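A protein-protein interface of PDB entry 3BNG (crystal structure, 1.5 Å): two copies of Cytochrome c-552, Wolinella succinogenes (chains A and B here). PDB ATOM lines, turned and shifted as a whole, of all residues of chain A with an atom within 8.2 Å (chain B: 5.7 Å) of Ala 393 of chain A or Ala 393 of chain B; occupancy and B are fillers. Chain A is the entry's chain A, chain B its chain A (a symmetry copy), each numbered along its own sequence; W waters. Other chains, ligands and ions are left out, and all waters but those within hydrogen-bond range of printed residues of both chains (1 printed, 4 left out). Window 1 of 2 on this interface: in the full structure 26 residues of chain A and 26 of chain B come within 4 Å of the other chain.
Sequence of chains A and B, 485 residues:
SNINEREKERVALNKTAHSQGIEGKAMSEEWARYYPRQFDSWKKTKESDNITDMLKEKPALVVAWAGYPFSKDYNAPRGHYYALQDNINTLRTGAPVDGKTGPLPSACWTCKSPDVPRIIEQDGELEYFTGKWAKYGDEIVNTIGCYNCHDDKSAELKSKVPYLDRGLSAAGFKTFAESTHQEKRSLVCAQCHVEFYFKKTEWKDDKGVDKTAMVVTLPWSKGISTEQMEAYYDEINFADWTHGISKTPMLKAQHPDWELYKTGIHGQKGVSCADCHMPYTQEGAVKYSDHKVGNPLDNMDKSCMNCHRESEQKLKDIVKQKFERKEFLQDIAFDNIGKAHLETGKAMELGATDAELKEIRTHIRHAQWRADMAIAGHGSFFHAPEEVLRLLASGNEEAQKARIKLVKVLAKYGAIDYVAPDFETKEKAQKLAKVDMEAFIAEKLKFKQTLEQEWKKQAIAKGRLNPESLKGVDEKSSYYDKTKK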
ATOM      1  N   ARG A 325     -14.005   0.750 -17.985  1.00  0.00           N
ATOM      2  CA  ARG A 325     -12.923   1.754 -17.971  1.00  0.00           C
ATOM      3  C   ARG A 325     -11.748   1.262 -18.787  1.00  0.00           C
ATOM      4  O   ARG A 325     -11.171   2.013 -19.617  1.00  0.00           O
ATOM      5  CB  ARG A 325     -12.440   2.057 -16.552  1.00  0.00           C
ATOM      6  CG  ARG A 325     -13.356   2.980 -15.823  1.00  0.00           C
ATOM      7  CD  ARG A 325     -12.690   3.477 -14.567  1.00  0.00           C
ATOM      8  NE  ARG A 325     -12.744   2.480 -13.524  1.00  0.00           N
ATOM      9  CZ  ARG A 325     -13.737   2.362 -12.646  1.00  0.00           C
ATOM     10  NH1 ARG A 325     -14.787   3.159 -12.691  1.00  0.00           N
ATOM     11  NH2 ARG A 325     -13.684   1.424 -11.757  1.00  0.00           N
ATOM     12  N   PHE A 328     -12.399   1.262 -22.569  1.00  0.00           N
ATOM     13  CA  PHE A 328     -12.377   2.645 -23.088  1.00  0.00           C
ATOM     14  C   PHE A 328     -10.947   3.052 -23.403  1.00  0.00           C
ATOM     15  O   PHE A 328     -10.637   3.498 -24.524  1.00  0.00           O
ATOM     16  CB  PHE A 328     -12.964   3.577 -22.009  1.00  0.00           C
ATOM     17  CG  PHE A 328     -12.876   5.036 -22.345  1.00  0.00           C
ATOM     18  CD1 PHE A 328     -13.680   5.587 -23.326  1.00  0.00           C
ATOM     19  CD2 PHE A 328     -12.007   5.882 -21.644  1.00  0.00           C
ATOM     20  CE1 PHE A 328     -13.603   6.971 -23.630  1.00  0.00           C
ATOM     21  CE2 PHE A 328     -11.924   7.238 -21.948  1.00  0.00           C
ATOM     22  CZ  PHE A 328     -12.728   7.791 -22.920  1.00  0.00           C
ATOM     23  N   LEU A 329     -10.059   2.831 -22.435  1.00  0.00           N
ATOM     24  CA  LEU A 329      -8.651   3.215 -22.624  1.00  0.00           C
ATOM     25  C   LEU A 329      -7.914   2.273 -23.573  1.00  0.00           C
ATOM     26  O   LEU A 329      -6.978   2.701 -24.260  1.00  0.00           O
ATOM     27  CB  LEU A 329      -7.908   3.379 -21.296  1.00  0.00           C
ATOM     28  CG  LEU A 329      -8.376   4.549 -20.419  1.00  0.00           C
ATOM     29  CD1 LEU A 329      -7.372   4.695 -19.286  1.00  0.00           C
ATOM     30  CD2 LEU A 329      -8.487   5.864 -21.140  1.00  0.00           C
ATOM     31  N   GLN A 330      -8.295   0.992 -23.563  1.00  0.00           N
ATOM     32  CA  GLN A 330      -7.655   0.013 -24.427  1.00  0.00           C
ATOM     33  C   GLN A 330      -7.956   0.384 -25.882  1.00  0.00           C
ATOM     34  O   GLN A 330      -7.081   0.344 -26.742  1.00  0.00           O
ATOM     35  CB  GLN A 330      -8.196  -1.386 -24.143  1.00  0.00           C
ATOM     36  CG  GLN A 330      -7.777  -2.392 -25.191  1.00  0.00           C
ATOM     37  CD  GLN A 330      -8.148  -3.835 -24.886  1.00  0.00           C
ATOM     38  OE1 GLN A 330      -8.023  -4.725 -25.763  1.00  0.00           O
ATOM     39  NE2 GLN A 330      -8.583  -4.086 -23.674  1.00  0.00           N
ATOM     40  N   ILE A 332      -8.705   3.259 -27.214  1.00  0.00           N
ATOM     41  CA  ILE A 332      -7.980   4.491 -27.597  1.00  0.00           C
ATOM     42  C   ILE A 332      -6.518   4.149 -27.845  1.00  0.00           C
ATOM     43  O   ILE A 332      -6.019   4.479 -28.900  1.00  0.00           O
ATOM     44  CB  ILE A 332      -8.075   5.596 -26.514  1.00  0.00           C
ATOM     45  CG1 ILE A 332      -9.487   6.178 -26.450  1.00  0.00           C
ATOM     46  CG2 ILE A 332      -7.000   6.688 -26.731  1.00  0.00           C
ATOM     47  CD1 ILE A 332      -9.712   6.961 -25.156  1.00  0.00           C
ATOM     48  N   ALA A 333      -5.847   3.466 -26.898  1.00  0.00           N
ATOM     49  CA  ALA A 333      -4.419   3.166 -27.054  1.00  0.00           C
ATOM     50  C   ALA A 333      -4.141   2.379 -28.337  1.00  0.00           C
ATOM     51  O   ALA A 333      -3.227   2.702 -29.087  1.00  0.00           O
ATOM     52  CB  ALA A 333      -3.865   2.416 -25.828  1.00  0.00           C
ATOM     53  N   ALA A 367       5.110   2.204 -26.472  1.00  0.00           N
ATOM     54  CA  ALA A 367       3.665   2.367 -26.426  1.00  0.00           C
ATOM     55  C   ALA A 367       2.996   0.990 -26.353  1.00  0.00           C
ATOM     56  O   ALA A 367       2.104   0.753 -25.521  1.00  0.00           O
ATOM     57  CB  ALA A 367       3.161   3.102 -27.690  1.00  0.00           C
ATOM     58  N   ARG A 370       3.728  -1.227 -23.224  1.00  0.00           N
ATOM     59  CA  ARG A 370       2.957  -0.794 -22.032  1.00  0.00           C
ATOM     60  C   ARG A 370       1.484  -1.185 -22.171  1.00  0.00           C
ATOM     61  O   ARG A 370       0.891  -1.724 -21.230  1.00  0.00           O
ATOM     62  CB  ARG A 370       3.143   0.711 -21.777  1.00  0.00           C
ATOM     63  CG  ARG A 370       4.567   1.066 -21.445  1.00  0.00           C
ATOM     64  CD  ARG A 370       4.823   2.561 -21.493  1.00  0.00           C
ATOM     65  NE  ARG A 370       6.268   2.807 -21.551  1.00  0.00           N
ATOM     66  CZ  ARG A 370       6.818   4.021 -21.469  1.00  0.00           C
ATOM     67  NH1 ARG A 370       6.046   5.105 -21.279  1.00  0.00           N
ATOM     68  NH2 ARG A 370       8.140   4.159 -21.623  1.00  0.00           N
ATOM     69  N   ALA A 371       0.904  -0.934 -23.354  1.00  0.00           N
ATOM     70  CA  ALA A 371      -0.504  -1.217 -23.545  1.00  0.00           C
ATOM     71  C   ALA A 371      -0.744  -2.747 -23.581  1.00  0.00           C
ATOM     72  O   ALA A 371      -1.756  -3.231 -23.078  1.00  0.00           O
ATOM     73  CB  ALA A 371      -1.000  -0.553 -24.835  1.00  0.00           C
ATOM     74  N   ALA A 374      -0.684  -4.132 -20.218  1.00  0.00           N
ATOM     75  CA  ALA A 374      -1.915  -3.800 -19.474  1.00  0.00           C
ATOM     76  C   ALA A 374      -3.075  -4.754 -19.803  1.00  0.00           C
ATOM     77  O   ALA A 374      -3.935  -5.009 -18.950  1.00  0.00           O
ATOM     78  CB  ALA A 374      -2.335  -2.388 -19.785  1.00  0.00           C
ATOM     79  N   GLU A 386      -5.954   0.165 -11.179  1.00  0.00           N
ATOM     80  CA  GLU A 386      -5.346   1.462 -11.328  1.00  0.00           C
ATOM     81  C   GLU A 386      -4.031   1.390 -12.126  1.00  0.00           C
ATOM     82  O   GLU A 386      -3.723   2.312 -12.883  1.00  0.00           O
ATOM     83  CB  GLU A 386      -5.191   2.150  -9.944  1.00  0.00           C
ATOM     84  CG  GLU A 386      -6.577   2.475  -9.373  1.00  0.00           C
ATOM     85  CD  GLU A 386      -6.635   2.803  -7.880  1.00  0.00           C
ATOM     86  OE1 GLU A 386      -5.703   3.455  -7.382  1.00  0.00           O
ATOM     87  OE2 GLU A 386      -7.651   2.383  -7.234  1.00  0.00           O
ATOM     88  N   GLU A 387      -3.255   0.338 -11.949  1.00  0.00           N
ATOM     89  CA  GLU A 387      -2.057   0.168 -12.746  1.00  0.00           C
ATOM     90  C   GLU A 387      -2.418  -0.072 -14.230  1.00  0.00           C
ATOM     91  O   GLU A 387      -1.769   0.491 -15.107  1.00  0.00           O
ATOM     92  CB  GLU A 387      -1.153  -0.931 -12.162  1.00  0.00           C
ATOM     93  CG  GLU A 387       0.077  -1.260 -12.971  1.00  0.00           C
ATOM     94  CD  GLU A 387       1.145  -0.150 -13.040  1.00  0.00           C
ATOM     95  OE1 GLU A 387       0.987   0.959 -12.479  1.00  0.00           O
ATOM     96  OE2 GLU A 387       2.201  -0.423 -13.668  1.00  0.00           O
ATOM     97  N   VAL A 388      -3.455  -0.877 -14.497  1.00  0.00           N
ATOM     98  CA  VAL A 388      -3.915  -1.113 -15.871  1.00  0.00           C
ATOM     99  C   VAL A 388      -4.274   0.221 -16.553  1.00  0.00           C
ATOM    100  O   VAL A 388      -3.806   0.496 -17.671  1.00  0.00           O
ATOM    101  CB  VAL A 388      -5.116  -2.086 -15.929  1.00  0.00           C
ATOM    102  CG1 VAL A 388      -5.816  -2.025 -17.280  1.00  0.00           C
ATOM    103  CG2 VAL A 388      -4.627  -3.478 -15.631  1.00  0.00           C
ATOM    104  N   LEU A 389      -5.068   1.062 -15.881  1.00  0.00           N
ATOM    105  CA  LEU A 389      -5.419   2.359 -16.484  1.00  0.00           C
ATOM    106  C   LEU A 389      -4.184   3.223 -16.703  1.00  0.00           C
ATOM    107  O   LEU A 389      -4.054   3.888 -17.746  1.00  0.00           O
ATOM    108  CB  LEU A 389      -6.474   3.125 -15.671  1.00  0.00           C
ATOM    109  CG  LEU A 389      -7.758   2.352 -15.332  1.00  0.00           C
ATOM    110  CD1 LEU A 389      -8.679   3.250 -14.535  1.00  0.00           C
ATOM    111  CD2 LEU A 389      -8.452   1.838 -16.598  1.00  0.00           C
ATOM    112  N   ARG A 390      -3.294   3.254 -15.710  1.00  0.00           N
ATOM    113  CA  ARG A 390      -2.099   4.102 -15.831  1.00  0.00           C
ATOM    114  C   ARG A 390      -1.248   3.594 -17.001  1.00  0.00           C
ATOM    115  O   ARG A 390      -0.708   4.392 -17.798  1.00  0.00           O
ATOM    116  CB  ARG A 390      -1.295   4.128 -14.525  1.00  0.00           C
ATOM    117  CG  ARG A 390      -0.152   5.167 -14.532  1.00  0.00           C
ATOM    118  CD  ARG A 390       0.940   4.806 -13.507  1.00  0.00           C
ATOM    119  NE  ARG A 390       1.562   3.547 -13.879  1.00  0.00           N
ATOM    120  CZ  ARG A 390       2.492   3.419 -14.827  1.00  0.00           C
ATOM    121  NH1 ARG A 390       2.981   4.487 -15.455  1.00  0.00           N
ATOM    122  NH2 ARG A 390       2.949   2.215 -15.131  1.00  0.00           N
ATOM    123  N   LEU A 391      -1.146   2.267 -17.134  1.00  0.00           N
ATOM    124  CA  LEU A 391      -0.327   1.716 -18.233  1.00  0.00           C
ATOM    125  C   LEU A 391      -0.944   2.035 -19.587  1.00  0.00           C
ATOM    126  O   LEU A 391      -0.222   2.299 -20.552  1.00  0.00           O
ATOM    127  CB  LEU A 391      -0.185   0.202 -18.115  1.00  0.00           C
ATOM    128  CG  LEU A 391       0.766  -0.267 -17.020  1.00  0.00           C
ATOM    129  CD1 LEU A 391       0.560  -1.781 -16.871  1.00  0.00           C
ATOM    130  CD2 LEU A 391       2.226   0.064 -17.351  1.00  0.00           C
ATOM    131  N   LEU A 392      -2.265   1.899 -19.688  1.00  0.00           N
ATOM    132  CA  LEU A 392      -2.918   2.231 -20.981  1.00  0.00           C
ATOM    133  C   LEU A 392      -2.771   3.716 -21.340  1.00  0.00           C
ATOM    134  O   LEU A 392      -2.636   4.094 -22.514  1.00  0.00           O
ATOM    135  CB  LEU A 392      -4.400   1.851 -20.958  1.00  0.00           C
ATOM    136  CG  LEU A 392      -4.673   0.351 -21.035  1.00  0.00           C
ATOM    137  CD1 LEU A 392      -6.104   0.026 -20.638  1.00  0.00           C
ATOM    138  CD2 LEU A 392      -4.345  -0.213 -22.442  1.00  0.00           C
ATOM    139  N   ALA A 393      -2.864   4.564 -20.326  1.00  0.00           N
ATOM    140  CA  ALA A 393      -2.635   6.000 -20.511  1.00  0.00           C
ATOM    141  C   ALA A 393      -1.215   6.290 -20.955  1.00  0.00           C
ATOM    142  O   ALA A 393      -0.987   7.105 -21.885  1.00  0.00           O
ATOM    143  CB  ALA A 393      -2.950   6.764 -19.241  1.00  0.00           C
ATOM    144  N   SER A 394      -0.260   5.619 -20.313  1.00  0.00           N
ATOM    145  CA  SER A 394       1.168   5.844 -20.615  1.00  0.00           C
ATOM    146  C   SER A 394       1.454   5.349 -22.038  1.00  0.00           C
ATOM    147  O   SER A 394       2.154   6.006 -22.809  1.00  0.00           O
ATOM    148  CB  SER A 394       2.063   5.083 -19.623  1.00  0.00           C
ATOM    149  OG  SER A 394       3.425   5.286 -19.960  1.00  0.00           O
ATOM    150  N   GLY A 395       0.916   4.182 -22.392  1.00  0.00           N
ATOM    151  CA  GLY A 395       1.128   3.632 -23.725  1.00  0.00           C
ATOM    152  C   GLY A 395       0.515   4.542 -24.784  1.00  0.00           C
ATOM    153  O   GLY A 395       1.107   4.811 -25.840  1.00  0.00           O
ATOM    154  N   ASN A 396      -0.695   5.000 -24.532  1.00  0.00           N
ATOM    155  CA  ASN A 396      -1.325   5.894 -25.477  1.00  0.00           C
ATOM    156  C   ASN A 396      -0.474   7.155 -25.699  1.00  0.00           C
ATOM    157  O   ASN A 396      -0.294   7.600 -26.825  1.00  0.00           O
ATOM    158  CB  ASN A 396      -2.704   6.323 -24.995  1.00  0.00           C
ATOM    159  CG  ASN A 396      -3.428   7.127 -26.052  1.00  0.00           C
ATOM    160  OD1 ASN A 396      -3.848   8.272 -25.817  1.00  0.00           O
ATOM    161  ND2 ASN A 396      -3.515   6.569 -27.236  1.00  0.00           N
ATOM    162  N   GLU A 397       0.026   7.738 -24.613  1.00  0.00           N
ATOM    163  CA  GLU A 397       0.877   8.920 -24.713  1.00  0.00           C
ATOM    164  C   GLU A 397       2.092   8.650 -25.602  1.00  0.00           C
ATOM    165  O   GLU A 397       2.411   9.494 -26.451  1.00  0.00           O
ATOM    166  CB  GLU A 397       1.336   9.417 -23.331  1.00  0.00           C
ATOM    167  CG  GLU A 397       2.408  10.542 -23.370  1.00  0.00           C
ATOM    168  CD  GLU A 397       1.945  11.844 -24.053  1.00  0.00           C
ATOM    169  OE1 GLU A 397       0.790  11.896 -24.537  1.00  0.00           O
ATOM    170  OE2 GLU A 397       2.748  12.849 -24.080  1.00  0.00           O
ATOM    171  N   GLU A 398       2.764   7.495 -25.424  1.00  0.00           N
ATOM    172  CA  GLU A 398       3.897   7.161 -26.294  1.00  0.00           C
ATOM    173  C   GLU A 398       3.461   7.058 -27.767  1.00  0.00           C
ATOM    174  O   GLU A 398       4.165   7.538 -28.663  1.00  0.00           O
ATOM    175  CB  GLU A 398       4.653   5.893 -25.852  1.00  0.00           C
ATOM    176  CG  GLU A 398       5.455   6.066 -24.552  1.00  0.00           C
ATOM    177  CD  GLU A 398       6.596   7.065 -24.762  1.00  0.00           C
ATOM    178  OE1 GLU A 398       7.401   6.880 -25.686  1.00  0.00           O
ATOM    179  OE2 GLU A 398       6.666   8.055 -24.022  1.00  0.00           O
ATOM    180  N   ALA A 399       2.304   6.446 -27.996  1.00  0.00           N
ATOM    181  CA  ALA A 399       1.797   6.272 -29.365  1.00  0.00           C
ATOM    182  C   ALA A 399       1.519   7.663 -29.972  1.00  0.00           C
ATOM    183  O   ALA A 399       1.841   7.916 -31.136  1.00  0.00           O
ATOM    184  CB  ALA A 399       0.530   5.412 -29.365  1.00  0.00           C
ATOM    185  N   GLN A 400       0.970   8.581 -29.172  1.00  0.00           N
ATOM    186  CA  GLN A 400       0.628   9.915 -29.690  1.00  0.00           C
ATOM    187  C   GLN A 400       1.881  10.738 -29.902  1.00  0.00           C
ATOM    188  O   GLN A 400       1.939  11.505 -30.872  1.00  0.00           O
ATOM    189  CB  GLN A 400      -0.372  10.622 -28.796  1.00  0.00           C
ATOM    190  CG  GLN A 400      -1.760   9.946 -28.842  1.00  0.00           C
ATOM    191  CD  GLN A 400      -2.568  10.273 -30.102  1.00  0.00           C
ATOM    192  OE1 GLN A 400      -3.665  10.850 -30.024  1.00  0.00           O
ATOM    193  NE2 GLN A 400      -2.066   9.878 -31.247  1.00  0.00           N
ATOM    194  N   LEU B 329      -0.029  11.154 -14.539  1.00  0.00           N
ATOM    195  CA  LEU B 329      -0.976  11.430 -15.630  1.00  0.00           C
ATOM    196  C   LEU B 329      -1.339  12.910 -15.725  1.00  0.00           C
ATOM    197  O   LEU B 329      -1.634  13.403 -16.821  1.00  0.00           O
ATOM    198  CB  LEU B 329      -2.222  10.544 -15.558  1.00  0.00           C
ATOM    199  CG  LEU B 329      -1.982   9.048 -15.802  1.00  0.00           C
ATOM    200  CD1 LEU B 329      -3.345   8.386 -15.936  1.00  0.00           C
ATOM    201  CD2 LEU B 329      -1.171   8.738 -17.029  1.00  0.00           C
ATOM    202  N   ILE B 332       1.443  14.783 -17.625  1.00  0.00           N
ATOM    203  CA  ILE B 332       1.377  14.496 -19.075  1.00  0.00           C
ATOM    204  C   ILE B 332       0.222  15.279 -19.683  1.00  0.00           C
ATOM    205  O   ILE B 332       0.447  15.987 -20.642  1.00  0.00           O
ATOM    206  CB  ILE B 332       1.190  12.987 -19.374  1.00  0.00           C
ATOM    207  CG1 ILE B 332       2.463  12.204 -19.049  1.00  0.00           C
ATOM    208  CG2 ILE B 332       0.715  12.756 -20.830  1.00  0.00           C
ATOM    209  CD1 ILE B 332       2.187  10.703 -18.951  1.00  0.00           C
ATOM    210  N   VAL B 388     -10.484   9.333 -11.757  1.00  0.00           N
ATOM    211  CA  VAL B 388      -9.464  10.373 -11.941  1.00  0.00           C
ATOM    212  C   VAL B 388      -8.466   9.956 -13.038  1.00  0.00           C
ATOM    213  O   VAL B 388      -8.199  10.737 -13.967  1.00  0.00           O
ATOM    214  CB  VAL B 388      -8.713  10.699 -10.628  1.00  0.00           C
ATOM    215  CG1 VAL B 388      -7.431  11.474 -10.898  1.00  0.00           C
ATOM    216  CG2 VAL B 388      -9.635  11.469  -9.721  1.00  0.00           C
ATOM    217  N   LEU B 389      -7.941   8.728 -12.959  1.00  0.00           N
ATOM    218  CA  LEU B 389      -7.000   8.278 -13.999  1.00  0.00           C
ATOM    219  C   LEU B 389      -7.664   8.234 -15.369  1.00  0.00           C
ATOM    220  O   LEU B 389      -7.057   8.628 -16.380  1.00  0.00           O
ATOM    221  CB  LEU B 389      -6.356   6.923 -13.669  1.00  0.00           C
ATOM    222  CG  LEU B 389      -5.690   6.810 -12.290  1.00  0.00           C
ATOM    223  CD1 LEU B 389      -5.111   5.420 -12.133  1.00  0.00           C
ATOM    224  CD2 LEU B 389      -4.608   7.879 -12.102  1.00  0.00           C
ATOM    225  N   ARG B 390      -8.893   7.717 -15.420  1.00  0.00           N
ATOM    226  CA  ARG B 390      -9.580   7.599 -16.715  1.00  0.00           C
ATOM    227  C   ARG B 390      -9.805   9.005 -17.285  1.00  0.00           C
ATOM    228  O   ARG B 390      -9.623   9.244 -18.498  1.00  0.00           O
ATOM    229  CB  ARG B 390     -10.900   6.831 -16.581  1.00  0.00           C
ATOM    230  CG  ARG B 390     -11.552   6.497 -17.942  1.00  0.00           C
ATOM    231  CD  ARG B 390     -13.066   6.252 -17.792  1.00  0.00           C
ATOM    232  NE  ARG B 390     -13.716   7.472 -17.344  1.00  0.00           N
ATOM    233  CZ  ARG B 390     -14.019   8.498 -18.139  1.00  0.00           C
ATOM    234  NH1 ARG B 390     -13.811   8.432 -19.453  1.00  0.00           N
ATOM    235  NH2 ARG B 390     -14.555   9.590 -17.616  1.00  0.00           N
ATOM    236  N   LEU B 391     -10.172   9.951 -16.414  1.00  0.00           N
ATOM    237  CA  LEU B 391     -10.420  11.322 -16.905  1.00  0.00           C
ATOM    238  C   LEU B 391      -9.135  11.962 -17.410  1.00  0.00           C
ATOM    239  O   LEU B 391      -9.156  12.704 -18.396  1.00  0.00           O
ATOM    240  CB  LEU B 391     -10.999  12.209 -15.807  1.00  0.00           C
ATOM    241  CG  LEU B 391     -12.463  11.942 -15.475  1.00  0.00           C
ATOM    242  CD1 LEU B 391     -12.773  12.714 -14.186  1.00  0.00           C
ATOM    243  CD2 LEU B 391     -13.394  12.370 -16.615  1.00  0.00           C
ATOM    244  N   LEU B 392      -8.043  11.770 -16.673  1.00  0.00           N
ATOM    245  CA  LEU B 392      -6.756  12.346 -17.143  1.00  0.00           C
ATOM    246  C   LEU B 392      -6.297  11.732 -18.472  1.00  0.00           C
ATOM    247  O   LEU B 392      -5.702  12.403 -19.331  1.00  0.00           O
ATOM    248  CB  LEU B 392      -5.661  12.172 -16.088  1.00  0.00           C
ATOM    249  CG  LEU B 392      -5.798  13.084 -14.872  1.00  0.00           C
ATOM    250  CD1 LEU B 392      -4.922  12.611 -13.723  1.00  0.00           C
ATOM    251  CD2 LEU B 392      -5.490  14.560 -15.234  1.00  0.00           C
ATOM    252  N   ALA B 393      -6.518  10.434 -18.612  1.00  0.00           N
ATOM    253  CA  ALA B 393      -6.228   9.742 -19.872  1.00  0.00           C
ATOM    254  C   ALA B 393      -7.079  10.269 -21.010  1.00  0.00           C
ATOM    255  O   ALA B 393      -6.570  10.513 -22.133  1.00  0.00           O
ATOM    256  CB  ALA B 393      -6.422   8.248 -19.723  1.00  0.00           C
ATOM    257  N   SER B 394      -8.367  10.463 -20.727  1.00  0.00           N
ATOM    258  CA  SER B 394      -9.315  10.926 -21.760  1.00  0.00           C
ATOM    259  C   SER B 394      -8.947  12.361 -22.158  1.00  0.00           C
ATOM    260  O   SER B 394      -8.946  12.710 -23.339  1.00  0.00           O
ATOM    261  CB  SER B 394     -10.757  10.901 -21.228  1.00  0.00           C
ATOM    262  OG  SER B 394     -11.640  11.387 -22.226  1.00  0.00           O
ATOM    263  N   GLY B 395      -8.636  13.202 -21.172  1.00  0.00           N
ATOM    264  CA  GLY B 395      -8.268  14.584 -21.452  1.00  0.00           C
ATOM    265  C   GLY B 395      -6.982  14.641 -22.268  1.00  0.00           C
ATOM    266  O   GLY B 395      -6.848  15.413 -23.230  1.00  0.00           O
ATOM    267  N   ASN B 396      -6.004  13.850 -21.875  1.00  0.00           N
ATOM    268  CA  ASN B 396      -4.766  13.828 -22.621  1.00  0.00           C
ATOM    269  C   ASN B 396      -5.010  13.438 -24.088  1.00  0.00           C
ATOM    270  O   ASN B 396      -4.458  14.043 -24.998  1.00  0.00           O
ATOM    271  CB  ASN B 396      -3.776  12.840 -22.019  1.00  0.00           C
ATOM    272  CG  ASN B 396      -2.428  12.932 -22.699  1.00  0.00           C
ATOM    273  OD1 ASN B 396      -1.903  11.938 -23.228  1.00  0.00           O
ATOM    274  ND2 ASN B 396      -1.896  14.130 -22.755  1.00  0.00           N
ATOM    275  N   GLU B 397      -5.822  12.407 -24.306  1.00  0.00           N
ATOM    276  CA  GLU B 397      -6.151  11.976 -25.662  1.00  0.00           C
ATOM    277  C   GLU B 397      -6.755  13.123 -26.473  1.00  0.00           C
ATOM    278  O   GLU B 397      -6.353  13.313 -27.630  1.00  0.00           O
ATOM    279  CB  GLU B 397      -7.104  10.769 -25.666  1.00  0.00           C
ATOM    280  CG  GLU B 397      -7.659  10.386 -27.067  1.00  0.00           C
ATOM    281  CD  GLU B 397      -6.583   9.963 -28.087  1.00  0.00           C
ATOM    282  OE1 GLU B 397      -5.379   9.981 -27.741  1.00  0.00           O
ATOM    283  OE2 GLU B 397      -6.957   9.574 -29.256  1.00  0.00           O
ATOM    284  N   GLU B 398      -7.700  13.884 -25.888  1.00  0.00           N
ATOM    285  CA  GLU B 398      -8.265  15.036 -26.602  1.00  0.00           C
ATOM    286  C   GLU B 398      -7.178  16.073 -26.940  1.00  0.00           C
ATOM    287  O   GLU B 398      -7.163  16.625 -28.046  1.00  0.00           O
ATOM    288  CB  GLU B 398      -9.445  15.693 -25.862  1.00  0.00           C
ATOM    289  CG  GLU B 398     -10.722  14.839 -25.839  1.00  0.00           C
ATOM    290  CD  GLU B 398     -11.278  14.679 -27.257  1.00  0.00           C
ATOM    291  OE1 GLU B 398     -11.508  15.690 -27.935  1.00  0.00           O
ATOM    292  OE2 GLU B 398     -11.454  13.537 -27.704  1.00  0.00           O
HETATM  293  O   HOH W   1      -6.205   9.912 -31.832  1.00  0.00           O
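The side-chain amide oxygen (OD1) of Asn 396 of chain A sits close to the side-chain carboxylate (OE1) of Glu 397 of chain B, 3.0 Å away. OD1 of Asn 396 of chain B sits close to OE1 of Glu 397 of chain A (3.0 Å). OE1 of Glu 397 of chain B sits close to OE1 of Gln 400 of chain A (3.0 Å).
CD of Arg 390 of chain B touches CG of Arg 325 of chain A (3.8 Å). Arg 390 of chain B touches Phe 328 of chain A (NH1 to CE2, 3.3 Å). Phe 328 of chain A touches Ser 394 of chain B. Leu 329 of chain A touches Ala 393 of chain B (CD2 to CB, 3.5 Å). Glu 397 of chain B touches Ile 332 of chain A. Glu 386 of chain A touches Leu 389 of chain B. CD2 of Leu 329 of chain B touches CB of Ala 393 of chain A, at 3.5 Å. Ala 393 of chain A touches Ala 393 of chain B (CB to CB, 3.8 Å). Glu 397 of chain A touches Ile 332 of chain B.
Of the printed residues of chain B, Leu 329 of chain A touches Ala 393. Glu 387 of chain A touches none of the printed residues of chain B. Ala 393 of chain A touches just these residues of chain B: Leu 329 and Ala 393. Printed residues of chain B within 4 Å of Gln 400 of chain A: Glu 397. Of the printed residues of chain A, Leu 389 of chain B touches Glu 386. Of chain A, only Leu 329 and Ala 393 come within 4 Å of Ala 393 of chain B. Printed residues of chain A within 4 Å of Ser 394 of chain B: Phe 328 (3.8 Å). The nearest residue of chain B that does not touch Ala 393 of chain A is Asn 396 of chain B (5.1 Å). The nearest printed residue of chain B that does not touch Leu 329 of chain A is Arg 390 of chain B (4.4 Å).
Printed residues of chain B that touch a printed residue of chain A: Leu 329, Ile 332, Leu 389, Arg 390, Ala 393, Ser 394, Asn 396 and Glu 397. Of the 25 printed residues of chain A, 9 touch a printed residue of chain B. Along chain A the printed residues that touch a printed residue of chain B span positions 325 to 400.
Leu 329 of chain A touches Ala 393 of chain B, and with the chains exchanged Ala 393 of chain A touches Leu 329 of chain B. Ile 332 of chain A touches Glu 397 of chain B, and with the chains exchanged Glu 397 of chain A touches Ile 332 of chain B. Ala 393 of chain A touches its own counterpart, Ala 393 of chain B. Asn 396 of chain A touches Glu 397 of chain B, and with the chains exchanged Glu 397 of chain A touches Asn 396 of chain B. 13 positions are printed for both chains. Of the 12 pairs that touch across the chains among the printed residues, 7 have their exchanged pair printed and touching as well.
Water W1 lies within hydrogen-bond range of the side-chain carboxylate (OE2) of Glu 397 of chain B (2.7 Å) and the side-chain amide oxygen (OE1) of Gln 400 of chain A (3.3 Å).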
